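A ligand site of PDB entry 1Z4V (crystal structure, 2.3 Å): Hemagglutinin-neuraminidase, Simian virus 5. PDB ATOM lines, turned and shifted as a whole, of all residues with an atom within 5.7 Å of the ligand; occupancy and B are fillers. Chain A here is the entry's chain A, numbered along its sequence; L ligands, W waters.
An oxygen (O5) of the ligand sits at hydrogen-bond distance from the side-chain carboxylate (OE1) of Glu 214 (2.6 Å).
NH2 of Arg 462 lies within salt-bridge range of O2 of the ligand, at 2.6 Å.
The side-chain hydroxyl of Tyr 490 lies close to an oxygen (O4) of the ligand.
O1 of the ligand is in salt-bridge range of NH1 of Arg 130, 3.0 Å away.
The guanidinium group of Arg 372 is in salt-bridge range of an oxygen (O2) of the ligand (3.1 Å).
The side-chain hydroxyl (OH) of Tyr 273 is in hydrogen-bond range of an oxygen (O6) of the ligand, 3.3 Å away.
O of Gly 428 is in hydrogen-bond range of NH2 of Arg 462, 2.7 Å away.
OH of Tyr 490 lies within hydrogen-bond range of NH1 of Arg 372.
OH of Tyr 490 sits at hydrogen-bond distance from OE2 of Glu 357, 2.8 Å away.
The side-chain carboxylate of Glu 357 lies within salt-bridge range of the guanidinium group of Arg 372.
NH2 of Arg 372 is in hydrogen-bond range of OD1 of Asn 374.
The backbone carbonyl oxygen (O) of Gly 428 lies within hydrogen-bond range of the guanidinium group (NH2) of Arg 372, 3.0 Å away.
The backbone NH (N) of Asn 255 lies within hydrogen-bond range of the backbone carbonyl oxygen (O) of Tyr 273, at 2.8 Å.
OD1 of Asn 374 is in hydrogen-bond range of N of Gly 428, at 3.3 Å.
Residues that only touch the ligand: Asn 255, Glu 357, Asn 374, Phe 208, Ile 131 and Phe 320.
Within 4 Å of the ligand: Arg 130, Ile 131, Phe 208, Glu 214, Asn 255, Tyr 273, Phe 320, Glu 357, Arg 372, Asn 374, Arg 462 and Tyr 490.
The nearest printed residue that does not touch the ligand is Ser 193 (4.2 Å).
Water W3 bridges an oxygen (O6) of the ligand and the backbone NH (N) of Glu 357.
Water W1 lies within hydrogen-bond range of an oxygen (O7) of the ligand (2.8 Å) and the side-chain hydroxyl of Tyr 218 (3.2 Å).
Water W4 bridges O8 of the ligand (2.8 Å) and OE1 of Glu 214 (3.2 Å).
Water W7 lies within hydrogen-bond range of an oxygen (O3) of the ligand (2.8 Å) and the backbone NH of Ser 193 (3.2 Å).
Water W6 lies within hydrogen-bond range of the side-chain carboxylate of Glu 357 (2.7 Å), the side-chain hydroxyl of Ser 193 (2.7 Å), the side-chain hydroxyl of Tyr 273 (2.7 Å) and a nitrogen (N1) of the ligand (2.9 Å).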
ATOM      1  N   ARG A 130      -3.749 -29.655 -13.816  1.00  0.00           N
ATOM      2  CA  ARG A 130      -4.745 -29.030 -14.679  1.00  0.00           C
ATOM      3  C   ARG A 130      -4.736 -27.520 -14.602  1.00  0.00           C
ATOM      4  O   ARG A 130      -4.052 -26.930 -13.765  1.00  0.00           O
ATOM      5  CB  ARG A 130      -6.158 -29.486 -14.312  1.00  0.00           C
ATOM      6  CG  ARG A 130      -6.545 -30.870 -14.823  1.00  0.00           C
ATOM      7  CD  ARG A 130      -8.078 -30.902 -14.988  1.00  0.00           C
ATOM      8  NE  ARG A 130      -8.525 -29.973 -16.026  1.00  0.00           N
ATOM      9  CZ  ARG A 130      -9.769 -29.537 -16.177  1.00  0.00           C
ATOM     10  NH1 ARG A 130     -10.735 -29.936 -15.346  1.00  0.00           N
ATOM     11  NH2 ARG A 130     -10.064 -28.702 -17.162  1.00  0.00           N
ATOM     12  N   ILE A 131      -5.533 -26.918 -15.486  1.00  0.00           N
ATOM     13  CA  ILE A 131      -5.727 -25.479 -15.550  1.00  0.00           C
ATOM     14  C   ILE A 131      -4.447 -24.690 -15.844  1.00  0.00           C
ATOM     15  O   ILE A 131      -3.939 -23.961 -14.993  1.00  0.00           O
ATOM     16  CB  ILE A 131      -6.359 -24.950 -14.237  1.00  0.00           C
ATOM     17  CG1 ILE A 131      -7.432 -25.928 -13.737  1.00  0.00           C
ATOM     18  CG2 ILE A 131      -7.001 -23.593 -14.478  1.00  0.00           C
ATOM     19  CD1 ILE A 131      -8.492 -26.277 -14.791  1.00  0.00           C
ATOM     20  N   LYS A 192      -6.536 -21.189  -6.783  1.00  0.00           N
ATOM     21  CA  LYS A 192      -7.188 -21.822  -7.929  1.00  0.00           C
ATOM     22  C   LYS A 192      -7.504 -20.875  -9.072  1.00  0.00           C
ATOM     23  O   LYS A 192      -7.425 -19.647  -8.933  1.00  0.00           O
ATOM     24  CB  LYS A 192      -8.507 -22.463  -7.495  1.00  0.00           C
ATOM     25  CG  LYS A 192      -8.396 -23.613  -6.517  1.00  0.00           C
ATOM     26  CD  LYS A 192      -7.839 -24.845  -7.201  1.00  0.00           C
ATOM     27  CE  LYS A 192      -8.140 -26.086  -6.380  1.00  0.00           C
ATOM     28  NZ  LYS A 192      -7.631 -27.308  -7.063  1.00  0.00           N
ATOM     29  N   SER A 193      -7.888 -21.481 -10.196  1.00  0.00           N
ATOM     30  CA  SER A 193      -8.280 -20.742 -11.397  1.00  0.00           C
ATOM     31  C   SER A 193      -7.311 -19.606 -11.724  1.00  0.00           C
ATOM     32  O   SER A 193      -7.696 -18.552 -12.196  1.00  0.00           O
ATOM     33  CB  SER A 193      -9.703 -20.208 -11.166  1.00  0.00           C
ATOM     34  OG  SER A 193     -10.363 -19.894 -12.362  1.00  0.00           O
ATOM     35  N   PHE A 208      -7.557 -16.969  -6.912  1.00  0.00           N
ATOM     36  CA  PHE A 208      -8.532 -16.767  -5.853  1.00  0.00           C
ATOM     37  C   PHE A 208      -8.307 -17.966  -4.942  1.00  0.00           C
ATOM     38  O   PHE A 208      -7.778 -18.977  -5.390  1.00  0.00           O
ATOM     39  CB  PHE A 208      -9.969 -16.724  -6.427  1.00  0.00           C
ATOM     40  CG  PHE A 208     -10.634 -18.068  -6.581  1.00  0.00           C
ATOM     41  CD1 PHE A 208     -11.397 -18.598  -5.553  1.00  0.00           C
ATOM     42  CD2 PHE A 208     -10.559 -18.751  -7.792  1.00  0.00           C
ATOM     43  CE1 PHE A 208     -12.109 -19.800  -5.719  1.00  0.00           C
ATOM     44  CE2 PHE A 208     -11.259 -19.954  -7.977  1.00  0.00           C
ATOM     45  CZ  PHE A 208     -12.030 -20.480  -6.943  1.00  0.00           C
ATOM     46  N   GLU A 214     -17.288 -24.997  -5.772  1.00  0.00           N
ATOM     47  CA  GLU A 214     -17.589 -23.830  -6.585  1.00  0.00           C
ATOM     48  C   GLU A 214     -19.006 -23.322  -6.437  1.00  0.00           C
ATOM     49  O   GLU A 214     -19.243 -22.118  -6.298  1.00  0.00           O
ATOM     50  CB  GLU A 214     -17.306 -24.128  -8.071  1.00  0.00           C
ATOM     51  CG  GLU A 214     -17.867 -23.085  -9.011  1.00  0.00           C
ATOM     52  CD  GLU A 214     -17.484 -23.330 -10.451  1.00  0.00           C
ATOM     53  OE1 GLU A 214     -17.543 -24.495 -10.875  1.00  0.00           O
ATOM     54  OE2 GLU A 214     -17.130 -22.353 -11.153  1.00  0.00           O
ATOM     55  N   TYR A 218     -21.084 -19.345  -5.148  1.00  0.00           N
ATOM     56  CA  TYR A 218     -22.143 -18.494  -5.681  1.00  0.00           C
ATOM     57  C   TYR A 218     -23.259 -18.194  -4.678  1.00  0.00           C
ATOM     58  O   TYR A 218     -23.833 -17.101  -4.690  1.00  0.00           O
ATOM     59  CB  TYR A 218     -22.717 -19.099  -6.956  1.00  0.00           C
ATOM     60  CG  TYR A 218     -21.759 -19.026  -8.128  1.00  0.00           C
ATOM     61  CD1 TYR A 218     -20.670 -19.888  -8.237  1.00  0.00           C
ATOM     62  CD2 TYR A 218     -21.894 -18.016  -9.101  1.00  0.00           C
ATOM     63  CE1 TYR A 218     -19.746 -19.761  -9.271  1.00  0.00           C
ATOM     64  CE2 TYR A 218     -20.972 -17.884 -10.143  1.00  0.00           C
ATOM     65  CZ  TYR A 218     -19.902 -18.759 -10.215  1.00  0.00           C
ATOM     66  OH  TYR A 218     -18.969 -18.613 -11.214  1.00  0.00           O
ATOM     67  N   ASN A 255     -13.525 -14.915 -10.034  1.00  0.00           N
ATOM     68  CA  ASN A 255     -12.434 -15.830 -10.395  1.00  0.00           C
ATOM     69  C   ASN A 255     -11.637 -15.286 -11.568  1.00  0.00           C
ATOM     70  O   ASN A 255     -12.166 -14.532 -12.385  1.00  0.00           O
ATOM     71  CB  ASN A 255     -12.960 -17.177 -10.901  1.00  0.00           C
ATOM     72  CG  ASN A 255     -13.722 -17.954  -9.872  1.00  0.00           C
ATOM     73  OD1 ASN A 255     -13.959 -17.494  -8.755  1.00  0.00           O
ATOM     74  ND2 ASN A 255     -14.105 -19.159 -10.240  1.00  0.00           N
ATOM     75  N   TYR A 273     -14.418 -13.491 -14.181  1.00  0.00           N
ATOM     76  CA  TYR A 273     -15.827 -13.868 -14.297  1.00  0.00           C
ATOM     77  C   TYR A 273     -16.330 -14.267 -12.907  1.00  0.00           C
ATOM     78  O   TYR A 273     -15.532 -14.514 -12.002  1.00  0.00           O
ATOM     79  CB  TYR A 273     -16.016 -14.991 -15.325  1.00  0.00           C
ATOM     80  CG  TYR A 273     -15.654 -16.390 -14.858  1.00  0.00           C
ATOM     81  CD1 TYR A 273     -14.348 -16.714 -14.532  1.00  0.00           C
ATOM     82  CD2 TYR A 273     -16.629 -17.371 -14.730  1.00  0.00           C
ATOM     83  CE1 TYR A 273     -14.008 -17.992 -14.102  1.00  0.00           C
ATOM     84  CE2 TYR A 273     -16.316 -18.657 -14.295  1.00  0.00           C
ATOM     85  CZ  TYR A 273     -15.003 -18.967 -13.987  1.00  0.00           C
ATOM     86  OH  TYR A 273     -14.673 -20.230 -13.544  1.00  0.00           O
ATOM     87  N   PHE A 320     -26.477 -21.686  -9.868  1.00  0.00           N
ATOM     88  CA  PHE A 320     -25.381 -20.978  -9.236  1.00  0.00           C
ATOM     89  C   PHE A 320     -25.891 -19.796  -8.401  1.00  0.00           C
ATOM     90  O   PHE A 320     -25.708 -18.632  -8.767  1.00  0.00           O
ATOM     91  CB  PHE A 320     -24.362 -20.478 -10.276  1.00  0.00           C
ATOM     92  CG  PHE A 320     -23.301 -21.499 -10.645  1.00  0.00           C
ATOM     93  CD1 PHE A 320     -23.175 -22.680  -9.935  1.00  0.00           C
ATOM     94  CD2 PHE A 320     -22.423 -21.254 -11.694  1.00  0.00           C
ATOM     95  CE1 PHE A 320     -22.183 -23.614 -10.256  1.00  0.00           C
ATOM     96  CE2 PHE A 320     -21.428 -22.186 -12.028  1.00  0.00           C
ATOM     97  CZ  PHE A 320     -21.306 -23.369 -11.305  1.00  0.00           C
ATOM     98  N   ALA A 356     -17.867 -16.261 -18.271  1.00  0.00           N
ATOM     99  CA  ALA A 356     -17.160 -17.535 -18.321  1.00  0.00           C
ATOM    100  C   ALA A 356     -15.658 -17.300 -18.223  1.00  0.00           C
ATOM    101  O   ALA A 356     -15.199 -16.167 -18.138  1.00  0.00           O
ATOM    102  CB  ALA A 356     -17.487 -18.264 -19.652  1.00  0.00           C
ATOM    103  N   GLU A 357     -14.892 -18.389 -18.224  1.00  0.00           N
ATOM    104  CA  GLU A 357     -13.437 -18.274 -18.200  1.00  0.00           C
ATOM    105  C   GLU A 357     -13.086 -17.519 -19.468  1.00  0.00           C
ATOM    106  O   GLU A 357     -13.915 -17.427 -20.387  1.00  0.00           O
ATOM    107  CB  GLU A 357     -12.784 -19.656 -18.236  1.00  0.00           C
ATOM    108  CG  GLU A 357     -13.047 -20.510 -17.020  1.00  0.00           C
ATOM    109  CD  GLU A 357     -12.474 -21.907 -17.172  1.00  0.00           C
ATOM    110  OE1 GLU A 357     -12.527 -22.443 -18.309  1.00  0.00           O
ATOM    111  OE2 GLU A 357     -11.964 -22.478 -16.175  1.00  0.00           O
ATOM    112  N   ARG A 372     -14.837 -18.126 -23.055  1.00  0.00           N
ATOM    113  CA  ARG A 372     -15.256 -19.519 -23.114  1.00  0.00           C
ATOM    114  C   ARG A 372     -16.769 -19.531 -23.375  1.00  0.00           C
ATOM    115  O   ARG A 372     -17.513 -18.684 -22.858  1.00  0.00           O
ATOM    116  CB  ARG A 372     -14.937 -20.217 -21.804  1.00  0.00           C
ATOM    117  CG  ARG A 372     -15.695 -21.515 -21.571  1.00  0.00           C
ATOM    118  CD  ARG A 372     -15.150 -22.245 -20.350  1.00  0.00           C
ATOM    119  NE  ARG A 372     -16.034 -23.332 -19.937  1.00  0.00           N
ATOM    120  CZ  ARG A 372     -15.714 -24.243 -19.012  1.00  0.00           C
ATOM    121  NH1 ARG A 372     -14.526 -24.199 -18.417  1.00  0.00           N
ATOM    122  NH2 ARG A 372     -16.601 -25.172 -18.670  1.00  0.00           N
ATOM    123  N   ASN A 374     -19.640 -21.050 -22.380  1.00  0.00           N
ATOM    124  CA  ASN A 374     -20.234 -21.878 -21.341  1.00  0.00           C
ATOM    125  C   ASN A 374     -21.745 -21.667 -21.328  1.00  0.00           C
ATOM    126  O   ASN A 374     -22.434 -22.147 -20.448  1.00  0.00           O
ATOM    127  CB  ASN A 374     -19.626 -21.500 -19.979  1.00  0.00           C
ATOM    128  CG  ASN A 374     -19.513 -22.685 -19.049  1.00  0.00           C
ATOM    129  OD1 ASN A 374     -19.076 -23.761 -19.453  1.00  0.00           O
ATOM    130  ND2 ASN A 374     -19.880 -22.491 -17.790  1.00  0.00           N
ATOM    131  N   LEU A 426     -25.171 -23.891 -18.960  1.00  0.00           N
ATOM    132  CA  LEU A 426     -24.030 -23.767 -18.064  1.00  0.00           C
ATOM    133  C   LEU A 426     -23.195 -25.016 -18.302  1.00  0.00           C
ATOM    134  O   LEU A 426     -23.087 -25.881 -17.424  1.00  0.00           O
ATOM    135  CB  LEU A 426     -24.504 -23.688 -16.621  1.00  0.00           C
ATOM    136  CG  LEU A 426     -23.456 -23.362 -15.551  1.00  0.00           C
ATOM    137  CD1 LEU A 426     -22.845 -21.981 -15.820  1.00  0.00           C
ATOM    138  CD2 LEU A 426     -24.118 -23.387 -14.188  1.00  0.00           C
ATOM    139  N   GLY A 428     -19.726 -26.546 -21.110  1.00  0.00           N
ATOM    140  CA  GLY A 428     -18.767 -26.246 -22.156  1.00  0.00           C
ATOM    141  C   GLY A 428     -17.346 -26.569 -21.712  1.00  0.00           C
ATOM    142  O   GLY A 428     -17.143 -27.281 -20.733  1.00  0.00           O
ATOM    143  N   VAL A 429     -16.361 -26.058 -22.462  1.00  0.00           N
ATOM    144  CA  VAL A 429     -14.939 -26.256 -22.151  1.00  0.00           C
ATOM    145  C   VAL A 429     -14.177 -25.047 -22.611  1.00  0.00           C
ATOM    146  O   VAL A 429     -14.629 -24.317 -23.488  1.00  0.00           O
ATOM    147  CB  VAL A 429     -14.284 -27.425 -22.923  1.00  0.00           C
ATOM    148  CG1 VAL A 429     -13.668 -28.404 -21.949  1.00  0.00           C
ATOM    149  CG2 VAL A 429     -15.264 -28.048 -23.888  1.00  0.00           C
ATOM    150  N   ARG A 462     -15.878 -34.797 -23.771  1.00  0.00           N
ATOM    151  CA  ARG A 462     -14.585 -34.107 -23.856  1.00  0.00           C
ATOM    152  C   ARG A 462     -13.652 -35.124 -24.474  1.00  0.00           C
ATOM    153  O   ARG A 462     -12.855 -35.757 -23.789  1.00  0.00           O
ATOM    154  CB  ARG A 462     -14.129 -33.661 -22.474  1.00  0.00           C
ATOM    155  CG  ARG A 462     -14.979 -32.532 -21.942  1.00  0.00           C
ATOM    156  CD  ARG A 462     -14.399 -31.912 -20.686  1.00  0.00           C
ATOM    157  NE  ARG A 462     -15.092 -30.670 -20.359  1.00  0.00           N
ATOM    158  CZ  ARG A 462     -14.755 -29.870 -19.353  1.00  0.00           C
ATOM    159  NH1 ARG A 462     -13.732 -30.165 -18.561  1.00  0.00           N
ATOM    160  NH2 ARG A 462     -15.456 -28.760 -19.149  1.00  0.00           N
ATOM    161  N   ALA A 489      -9.155 -31.991 -22.366  1.00  0.00           N
ATOM    162  CA  ALA A 489      -9.937 -30.954 -21.719  1.00  0.00           C
ATOM    163  C   ALA A 489      -9.626 -29.588 -22.334  1.00  0.00           C
ATOM    164  O   ALA A 489      -9.963 -29.370 -23.499  1.00  0.00           O
ATOM    165  CB  ALA A 489      -9.678 -30.962 -20.217  1.00  0.00           C
ATOM    166  N   TYR A 490      -9.001 -28.682 -21.566  1.00  0.00           N
ATOM    167  CA  TYR A 490      -8.682 -27.329 -22.053  1.00  0.00           C
ATOM    168  C   TYR A 490      -7.587 -27.307 -23.112  1.00  0.00           C
ATOM    169  O   TYR A 490      -6.768 -28.210 -23.201  1.00  0.00           O
ATOM    170  CB  TYR A 490      -8.223 -26.411 -20.904  1.00  0.00           C
ATOM    171  CG  TYR A 490      -9.272 -26.092 -19.877  1.00  0.00           C
ATOM    172  CD1 TYR A 490     -10.519 -26.711 -19.904  1.00  0.00           C
ATOM    173  CD2 TYR A 490      -9.010 -25.170 -18.872  1.00  0.00           C
ATOM    174  CE1 TYR A 490     -11.495 -26.416 -18.961  1.00  0.00           C
ATOM    175  CE2 TYR A 490      -9.979 -24.861 -17.911  1.00  0.00           C
ATOM    176  CZ  TYR A 490     -11.210 -25.480 -17.970  1.00  0.00           C
ATOM    177  OH  TYR A 490     -12.152 -25.096 -17.058  1.00  0.00           O
HETATM  178  C1  LIG L   1     -13.863 -27.421 -16.292  1.00  0.00           C
HETATM  179  C2  LIG L   1     -13.653 -26.510 -15.223  1.00  0.00           C
HETATM  180  C3  LIG L   1     -12.425 -26.642 -14.368  1.00  0.00           C
HETATM  181  C4  LIG L   1     -12.218 -25.396 -13.468  1.00  0.00           C
HETATM  182  C5  LIG L   1     -13.532 -24.816 -13.010  1.00  0.00           C
HETATM  183  C6  LIG L   1     -14.339 -24.426 -14.259  1.00  0.00           C
HETATM  184  C7  LIG L   1     -15.727 -23.855 -13.878  1.00  0.00           C
HETATM  185  C8  LIG L   1     -16.549 -23.415 -15.089  1.00  0.00           C
HETATM  186  C9  LIG L   1     -17.924 -22.865 -14.676  1.00  0.00           C
HETATM  187  C10 LIG L   1     -13.582 -23.516 -10.900  1.00  0.00           C
HETATM  188  C11 LIG L   1     -13.211 -22.252 -10.170  1.00  0.00           C
HETATM  189  N1  LIG L   1     -13.237 -23.650 -12.174  1.00  0.00           N
HETATM  190  O1  LIG L   1     -13.041 -28.481 -16.525  1.00  0.00           O
HETATM  191  O2  LIG L   1     -14.868 -27.241 -17.092  1.00  0.00           O
HETATM  192  O3  LIG L   1     -11.422 -25.792 -12.358  1.00  0.00           O
HETATM  193  O4  LIG L   1     -14.578 -25.606 -15.064  1.00  0.00           O
HETATM  194  O5  LIG L   1     -16.504 -24.862 -13.226  1.00  0.00           O
HETATM  195  O6  LIG L   1     -15.826 -22.381 -15.777  1.00  0.00           O
HETATM  196  O7  LIG L   1     -17.866 -21.785 -13.762  1.00  0.00           O
HETATM  197  O8  LIG L   1     -14.251 -24.485 -10.217  1.00  0.00           O
HETATM  198  O   HOH W   1     -19.776 -19.766 -14.118  1.00  0.00           O
HETATM  199  O   HOH W   2     -17.211 -26.859 -15.223  1.00  0.00           O
HETATM  200  O   HOH W   3     -16.845 -20.613 -17.672  1.00  0.00           O
HETATM  201  O   HOH W   4     -15.574 -26.957 -10.204  1.00  0.00           O
HETATM  202  O   HOH W   5     -13.797 -24.245  -7.433  1.00  0.00           O
HETATM  203  O   HOH W   6     -12.206 -21.396 -13.712  1.00  0.00           O
HETATM  204  O   HOH W   7     -10.105 -23.689 -11.012  1.00  0.00           O
